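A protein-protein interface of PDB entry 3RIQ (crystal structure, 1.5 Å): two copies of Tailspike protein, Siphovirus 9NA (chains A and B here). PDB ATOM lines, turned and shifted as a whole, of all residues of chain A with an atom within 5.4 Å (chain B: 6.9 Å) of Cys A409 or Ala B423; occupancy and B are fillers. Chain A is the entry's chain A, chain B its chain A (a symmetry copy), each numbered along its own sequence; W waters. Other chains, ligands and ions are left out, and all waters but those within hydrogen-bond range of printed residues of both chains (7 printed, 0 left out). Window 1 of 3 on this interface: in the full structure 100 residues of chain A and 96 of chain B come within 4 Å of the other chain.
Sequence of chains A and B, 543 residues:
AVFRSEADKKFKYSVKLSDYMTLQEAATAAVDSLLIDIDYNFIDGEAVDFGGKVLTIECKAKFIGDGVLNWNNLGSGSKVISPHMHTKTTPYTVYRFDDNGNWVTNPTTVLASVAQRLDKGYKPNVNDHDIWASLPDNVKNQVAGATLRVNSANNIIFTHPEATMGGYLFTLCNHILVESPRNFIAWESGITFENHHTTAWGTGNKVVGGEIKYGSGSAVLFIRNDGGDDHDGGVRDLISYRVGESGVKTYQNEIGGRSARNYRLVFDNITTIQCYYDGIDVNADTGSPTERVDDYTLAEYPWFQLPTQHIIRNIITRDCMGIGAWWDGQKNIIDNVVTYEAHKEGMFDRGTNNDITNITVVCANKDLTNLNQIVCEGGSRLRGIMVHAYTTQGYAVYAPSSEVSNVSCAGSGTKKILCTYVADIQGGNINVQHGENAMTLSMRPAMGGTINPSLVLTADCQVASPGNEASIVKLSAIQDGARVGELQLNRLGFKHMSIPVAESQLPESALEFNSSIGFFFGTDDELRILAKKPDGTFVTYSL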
ATOM      1  N   VAL A 387      17.733 -22.049  17.109  1.00  0.00           N
ATOM      2  CA  VAL A 387      16.778 -21.051  17.576  1.00  0.00           C
ATOM      3  C   VAL A 387      17.371 -20.263  18.746  1.00  0.00           C
ATOM      4  O   VAL A 387      18.013 -20.837  19.632  1.00  0.00           O
ATOM      5  CB  VAL A 387      15.489 -21.752  18.033  1.00  0.00           C
ATOM      6  CG1 VAL A 387      14.521 -20.778  18.710  1.00  0.00           C
ATOM      7  CG2 VAL A 387      14.788 -22.401  16.819  1.00  0.00           C
ATOM      8  N   ALA A 396      10.293 -23.445  20.816  1.00  0.00           N
ATOM      9  CA  ALA A 396      11.347 -23.202  19.830  1.00  0.00           C
ATOM     10  C   ALA A 396      11.021 -23.868  18.490  1.00  0.00           C
ATOM     11  O   ALA A 396      11.152 -23.237  17.422  1.00  0.00           O
ATOM     12  CB  ALA A 396      12.691 -23.707  20.355  1.00  0.00           C
ATOM     13  N   VAL A 407      19.459 -29.957  16.306  1.00  0.00           N
ATOM     14  CA  VAL A 407      18.740 -28.785  16.785  1.00  0.00           C
ATOM     15  C   VAL A 407      19.442 -28.212  18.007  1.00  0.00           C
ATOM     16  O   VAL A 407      19.852 -28.954  18.913  1.00  0.00           O
ATOM     17  CB  VAL A 407      17.255 -29.119  17.169  1.00  0.00           C
ATOM     18  CG1 VAL A 407      16.523 -27.874  17.575  1.00  0.00           C
ATOM     19  CG2 VAL A 407      16.563 -29.758  16.036  1.00  0.00           C
ATOM     20  N   SER A 408      19.564 -26.888  18.025  1.00  0.00           N
ATOM     21  CA  SER A 408      20.161 -26.157  19.124  1.00  0.00           C
ATOM     22  C   SER A 408      19.267 -24.979  19.502  1.00  0.00           C
ATOM     23  O   SER A 408      18.807 -24.245  18.604  1.00  0.00           O
ATOM     24  CB  SER A 408      21.567 -25.675  18.675  1.00  0.00           C
ATOM     25  OG  SER A 408      22.116 -24.795  19.619  1.00  0.00           O
ATOM     26  N   CYS A 409      18.996 -24.814  20.810  1.00  0.00           N
ATOM     27  CA  CYS A 409      18.206 -23.684  21.298  1.00  0.00           C
ATOM     28  C   CYS A 409      19.046 -22.865  22.242  1.00  0.00           C
ATOM     29  O   CYS A 409      19.477 -23.377  23.296  1.00  0.00           O
ATOM     30  CB  CYS A 409      16.923 -24.150  22.005  1.00  0.00           C
ATOM     31  SG  CYS A 409      15.927 -25.234  20.972  1.00  0.00           S
ATOM     32  N   ALA A 410      19.298 -21.615  21.889  1.00  0.00           N
ATOM     33  CA  ALA A 410      20.272 -20.783  22.620  1.00  0.00           C
ATOM     34  C   ALA A 410      19.628 -19.954  23.711  1.00  0.00           C
ATOM     35  O   ALA A 410      18.388 -19.837  23.811  1.00  0.00           O
ATOM     36  CB  ALA A 410      21.005 -19.845  21.636  1.00  0.00           C
ATOM     37  N   GLY A 411      20.488 -19.386  24.555  1.00  0.00           N
ATOM     38  CA  GLY A 411      20.063 -18.370  25.518  1.00  0.00           C
ATOM     39  C   GLY A 411      19.156 -18.923  26.597  1.00  0.00           C
ATOM     40  O   GLY A 411      19.276 -20.099  26.975  1.00  0.00           O
ATOM     41  N   THR A 414      12.519 -19.826  25.217  1.00  0.00           N
ATOM     42  CA  THR A 414      11.958 -21.170  25.082  1.00  0.00           C
ATOM     43  C   THR A 414      12.936 -22.084  24.335  1.00  0.00           C
ATOM     44  O   THR A 414      13.609 -21.677  23.362  1.00  0.00           O
ATOM     45  CB  THR A 414      10.594 -21.168  24.374  1.00  0.00           C
ATOM     46  OG1 THR A 414      10.138 -22.523  24.274  1.00  0.00           O
ATOM     47  CG2 THR A 414      10.659 -20.504  22.965  1.00  0.00           C
ATOM     48  N   LYS A 415      13.017 -23.321  24.834  1.00  0.00           N
ATOM     49  CA  LYS A 415      13.838 -24.375  24.236  1.00  0.00           C
ATOM     50  C   LYS A 415      13.011 -25.625  23.959  1.00  0.00           C
ATOM     51  O   LYS A 415      13.568 -26.691  23.699  1.00  0.00           O
ATOM     52  CB  LYS A 415      15.015 -24.746  25.156  1.00  0.00           C
ATOM     53  CG  LYS A 415      15.714 -23.578  25.825  1.00  0.00           C
ATOM     54  CD  LYS A 415      17.116 -23.982  26.274  1.00  0.00           C
ATOM     55  CE  LYS A 415      17.416 -23.419  27.642  1.00  0.00           C
ATOM     56  NZ  LYS A 415      16.997 -22.001  27.690  1.00  0.00           N
ATOM     57  N   LYS A 416      11.682 -25.491  23.981  1.00  0.00           N
ATOM     58  CA  LYS A 416      10.804 -26.630  23.787  1.00  0.00           C
ATOM     59  C   LYS A 416      10.745 -27.087  22.336  1.00  0.00           C
ATOM     60  O   LYS A 416      10.558 -26.278  21.416  1.00  0.00           O
ATOM     61  CB  LYS A 416       9.377 -26.303  24.287  1.00  0.00           C
ATOM     62  CG  LYS A 416       9.297 -25.968  25.782  1.00  0.00           C
ATOM     63  CD  LYS A 416       7.825 -25.738  26.236  1.00  0.00           C
ATOM     64  CE  LYS A 416       7.760 -25.385  27.734  1.00  0.00           C
ATOM     65  NZ  LYS A 416       8.617 -24.199  28.067  1.00  0.00           N
ATOM     66  N   ILE A 417      10.881 -28.394  22.155  1.00  0.00           N
ATOM     67  CA  ILE A 417      10.814 -29.060  20.839  1.00  0.00           C
ATOM     68  C   ILE A 417       9.700 -30.107  20.879  1.00  0.00           C
ATOM     69  O   ILE A 417       9.724 -31.042  21.715  1.00  0.00           O
ATOM     70  CB  ILE A 417      12.153 -29.781  20.507  1.00  0.00           C
ATOM     71  CG1 ILE A 417      13.312 -28.781  20.518  1.00  0.00           C
ATOM     72  CG2 ILE A 417      12.020 -30.543  19.185  1.00  0.00           C
ATOM     73  CD1 ILE A 417      14.685 -29.388  20.413  1.00  0.00           C
ATOM     74  N   GLU B 403      27.748 -14.857  24.951  1.00  0.00           N
ATOM     75  CA  GLU B 403      27.132 -16.173  25.060  1.00  0.00           C
ATOM     76  C   GLU B 403      27.325 -16.954  23.768  1.00  0.00           C
ATOM     77  O   GLU B 403      27.402 -16.372  22.683  1.00  0.00           O
ATOM     78  CB  GLU B 403      25.671 -16.062  25.436  1.00  0.00           C
ATOM     79  CG  GLU B 403      24.807 -15.407  24.408  1.00  0.00           C
ATOM     80  CD  GLU B 403      23.372 -15.334  24.891  1.00  0.00           C
ATOM     81  OE1 GLU B 403      22.809 -16.386  25.272  1.00  0.00           O
ATOM     82  OE2 GLU B 403      22.798 -14.238  24.906  1.00  0.00           O
ATOM     83  N   VAL B 404      27.415 -18.270  23.904  1.00  0.00           N
ATOM     84  CA  VAL B 404      27.715 -19.164  22.796  1.00  0.00           C
ATOM     85  C   VAL B 404      26.701 -20.319  22.758  1.00  0.00           C
ATOM     86  O   VAL B 404      26.226 -20.755  23.801  1.00  0.00           O
ATOM     87  CB  VAL B 404      29.148 -19.736  22.981  1.00  0.00           C
ATOM     88  CG1 VAL B 404      29.578 -20.507  21.773  1.00  0.00           C
ATOM     89  CG2 VAL B 404      30.158 -18.623  23.236  1.00  0.00           C
ATOM     90  N   SER B 405      26.401 -20.808  21.561  1.00  0.00           N
ATOM     91  CA  SER B 405      25.586 -22.018  21.388  1.00  0.00           C
ATOM     92  C   SER B 405      26.075 -22.774  20.157  1.00  0.00           C
ATOM     93  O   SER B 405      26.566 -22.166  19.198  1.00  0.00           O
ATOM     94  CB  SER B 405      24.111 -21.662  21.255  1.00  0.00           C
ATOM     95  OG  SER B 405      23.910 -20.934  20.069  1.00  0.00           O
ATOM     96  N   ASN B 406      25.981 -24.107  20.206  1.00  0.00           N
ATOM     97  CA  ASN B 406      26.355 -24.982  19.080  1.00  0.00           C
ATOM     98  C   ASN B 406      27.801 -24.760  18.656  1.00  0.00           C
ATOM     99  O   ASN B 406      28.071 -24.302  17.551  1.00  0.00           O
ATOM    100  CB  ASN B 406      25.381 -24.847  17.901  1.00  0.00           C
ATOM    101  CG  ASN B 406      25.660 -25.869  16.805  1.00  0.00           C
ATOM    102  OD1 ASN B 406      26.218 -26.910  17.069  1.00  0.00           O
ATOM    103  ND2 ASN B 406      25.337 -25.534  15.559  1.00  0.00           N
ATOM    104  N   CYS B 419      33.558 -17.974  28.191  1.00  0.00           N
ATOM    105  CA  CYS B 419      32.429 -17.083  27.909  1.00  0.00           C
ATOM    106  C   CYS B 419      31.523 -16.990  29.097  1.00  0.00           C
ATOM    107  O   CYS B 419      31.813 -17.583  30.133  1.00  0.00           O
ATOM    108  CB  CYS B 419      31.647 -17.541  26.655  1.00  0.00           C
ATOM    109  SG  CYS B 419      30.879 -19.131  26.917  1.00  0.00           S
ATOM    110  N   TYR B 421      28.041 -17.603  29.071  1.00  0.00           N
ATOM    111  CA  TYR B 421      26.978 -18.605  29.040  1.00  0.00           C
ATOM    112  C   TYR B 421      27.194 -19.532  27.839  1.00  0.00           C
ATOM    113  O   TYR B 421      27.434 -19.047  26.720  1.00  0.00           O
ATOM    114  CB  TYR B 421      25.587 -17.918  28.945  1.00  0.00           C
ATOM    115  CG  TYR B 421      24.471 -18.935  28.881  1.00  0.00           C
ATOM    116  CD1 TYR B 421      24.039 -19.608  30.052  1.00  0.00           C
ATOM    117  CD2 TYR B 421      23.874 -19.280  27.664  1.00  0.00           C
ATOM    118  CE1 TYR B 421      23.029 -20.588  29.992  1.00  0.00           C
ATOM    119  CE2 TYR B 421      22.874 -20.268  27.608  1.00  0.00           C
ATOM    120  CZ  TYR B 421      22.454 -20.900  28.759  1.00  0.00           C
ATOM    121  OH  TYR B 421      21.486 -21.886  28.672  1.00  0.00           O
ATOM    122  N   VAL B 422      27.083 -20.835  28.095  1.00  0.00           N
ATOM    123  CA  VAL B 422      27.171 -21.877  27.078  1.00  0.00           C
ATOM    124  C   VAL B 422      25.789 -22.551  27.033  1.00  0.00           C
ATOM    125  O   VAL B 422      25.305 -23.039  28.057  1.00  0.00           O
ATOM    126  CB  VAL B 422      28.279 -22.919  27.442  1.00  0.00           C
ATOM    127  CG1 VAL B 422      28.235 -24.097  26.508  1.00  0.00           C
ATOM    128  CG2 VAL B 422      29.686 -22.282  27.419  1.00  0.00           C
ATOM    129  N   ALA B 423      25.164 -22.584  25.863  1.00  0.00           N
ATOM    130  CA  ALA B 423      23.802 -23.108  25.736  1.00  0.00           C
ATOM    131  C   ALA B 423      23.701 -24.625  25.820  1.00  0.00           C
ATOM    132  O   ALA B 423      24.683 -25.345  25.620  1.00  0.00           O
ATOM    133  CB  ALA B 423      23.197 -22.636  24.403  1.00  0.00           C
ATOM    134  N   ASP B 424      22.485 -25.080  26.088  1.00  0.00           N
ATOM    135  CA  ASP B 424      22.185 -26.499  26.197  1.00  0.00           C
ATOM    136  C   ASP B 424      22.471 -27.263  24.895  1.00  0.00           C
ATOM    137  O   ASP B 424      22.370 -26.723  23.793  1.00  0.00           O
ATOM    138  CB  ASP B 424      20.693 -26.711  26.545  1.00  0.00           C
ATOM    139  CG  ASP B 424      20.280 -26.144  27.911  1.00  0.00           C
ATOM    140  OD1 ASP B 424      21.094 -25.545  28.640  1.00  0.00           O
ATOM    141  OD2 ASP B 424      19.086 -26.328  28.256  1.00  0.00           O
ATOM    142  N   ILE B 425      22.839 -28.534  25.043  1.00  0.00           N
ATOM    143  CA  ILE B 425      22.821 -29.523  23.962  1.00  0.00           C
ATOM    144  C   ILE B 425      21.492 -30.276  24.006  1.00  0.00           C
ATOM    145  O   ILE B 425      21.080 -30.754  25.075  1.00  0.00           O
ATOM    146  CB  ILE B 425      23.979 -30.525  24.178  1.00  0.00           C
ATOM    147  CG1 ILE B 425      25.330 -29.796  24.008  1.00  0.00           C
ATOM    148  CG2 ILE B 425      23.860 -31.729  23.249  1.00  0.00           C
ATOM    149  CD1 ILE B 425      26.525 -30.629  24.437  1.00  0.00           C
ATOM    150  N   GLN B 426      20.816 -30.359  22.857  1.00  0.00           N
ATOM    151  CA  GLN B 426      19.526 -31.073  22.709  1.00  0.00           C
ATOM    152  C   GLN B 426      19.589 -32.073  21.566  1.00  0.00           C
ATOM    153  O   GLN B 426      20.396 -31.927  20.619  1.00  0.00           O
ATOM    154  CB  GLN B 426      18.356 -30.092  22.526  1.00  0.00           C
ATOM    155  CG  GLN B 426      18.133 -29.328  23.858  1.00  0.00           C
ATOM    156  CD  GLN B 426      17.098 -28.238  23.755  1.00  0.00           C
ATOM    157  OE1 GLN B 426      17.424 -27.045  23.813  1.00  0.00           O
ATOM    158  NE2 GLN B 426      15.846 -28.631  23.583  1.00  0.00           N
HETATM  159  O   HOH W   1      22.013 -29.084  20.499  1.00  0.00           O
HETATM  160  O   HOH W   2      23.287 -26.277  21.428  1.00  0.00           O
HETATM  161  O   HOH W   3      23.442 -18.882  24.071  1.00  0.00           O
HETATM  162  O   HOH W   4      20.322 -23.038  25.904  1.00  0.00           O
HETATM  163  O   HOH W   5      19.946 -32.285  17.979  1.00  0.00           O
HETATM  164  O   HOH W   6      19.848 -26.817  22.497  1.00  0.00           O
HETATM  165  O   HOH W   7      21.435 -22.021  18.454  1.00  0.00           O
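Of the 11 printed residues of chain A, 7 touch a printed residue of chain B. Hydrophobic or aromatic side chains of chain A that line the printed part of chain B: Ala A410 and Ile A417. Printed residues of chain B that touch a printed residue of chain A: Glu B403, Ser B405, Asn B406, Tyr B421, Ala B423, Asp B424 and Gln B426. Hydrophobic or aromatic side chains of chain B that line the printed part of chain A: Tyr B421 and Ala B423. Among the printed residues, 11 pairs touch across the chains. Among the printed residues, no Asp or Glu carboxylate lies within 4 Å of a Lys or Arg side-chain nitrogen of the other chain.
No position is printed for both chains. Of the 11 pairs that touch across the chains among the printed residues, none has its exchanged pair printed and touching as well.
Water W2 lies within hydrogen-bond range of the backbone carbonyl oxygen (O) of Asp B424 and the side-chain hydroxyl (OG) of Ser A408. Water W1 lies within hydrogen-bond range of O of Val A407 and N of Gln B426. Water W6 lies within hydrogen-bond range of N of Cys A409, OE1 of Gln B426 and O of Asp B424. Water W4 lies within hydrogen-bond range of the backbone carbonyl oxygen of Cys A409 (2.8 Å), the backbone NH of Asp B424 (3.0 Å), the side-chain hydroxyl of Tyr B421 (3.2 Å) and the backbone carbonyl oxygen of Gly A411 (3.3 Å). Water W3 lies within hydrogen-bond range of OE1 of Glu B403 (2.8 Å), N of Gly A411 (3.0 Å) and O of Val B404 (3.4 Å). Water W7 lies within hydrogen-bond range of the side-chain hydroxyl of Ser A408 and the side-chain hydroxyl of Ser B405.
The backbone carbonyl oxygen of Ser A408 sits at hydrogen-bond distance from the backbone NH of Val A387. N of Ala A410 sits at hydrogen-bond distance from O of Val A387, at 2.7 Å. The backbone carbonyl oxygen (O) of Gly A411 is in hydrogen-bond range of the side-chain amino group (NZ) of Lys A415. O of Tyr B421 lies within hydrogen-bond range of N of Val B404, at 2.9 Å. The backbone carbonyl oxygen (O) of Val B404 lies within hydrogen-bond range of the backbone NH (N) of Ala B423 (3.0 Å). O of Tyr B421 sits at hydrogen-bond distance from SG of Cys B419 (3.5 Å).
Among the printed residues, pairs that only touch across the chains: Gly A411 with Glu B403 (3.4 Å), Lys A415 with Asp B424 (3.4 Å), Ile A417 with Gln B426 (3.5 Å), Ala A410 with Ser B405 (3.5 Å), Ser A408 with Asn B406 (3.7 Å), Ala A410 with Ala B423 (3.9 Å) and Cys A409 with Ala B423 (3.95 Å).
Of the printed residues of chain B, Ser A408 touches Asn B406 (3.7 Å). Of the printed residues of chain B, Gly A411 touches Glu B403 (3.4 Å) and Tyr B421 (3.3 Å). Thr A414 touches none of the printed residues of chain B. Of the printed residues of chain B, Ile A417 touches Gln B426 (3.5 Å). Of the printed residues of chain A, Glu B403 touches Gly A411. Printed residues of chain A within 4 Å of Ser B405: Ala A410 (3.5 Å). Ala B423 touches two residues of chain A. Ile B425 touches none of the printed residues of chain A. The nearest residue of chain A that does not touch Ala B423 is Gly A411 (4.2 Å). The nearest printed residue of chain B that does not touch Gly A411 is Ala B423 (4.2 Å).
The side-chain sulfur (SG) of Cys A409 sits close to the side-chain amide oxygen (OE1) of Gln B426 (3.7 Å). OH of Tyr B421 is in hydrogen-bond range of O of Gly A411. The side-chain amide nitrogen of Gln B426 is in hydrogen-bond range of the backbone carbonyl oxygen of Lys A415, 3.0 Å away. The backbone carbonyl oxygen (O) of Val A407 sits close to the backbone carbonyl oxygen (O) of Gln B426, 3.5 Å away.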
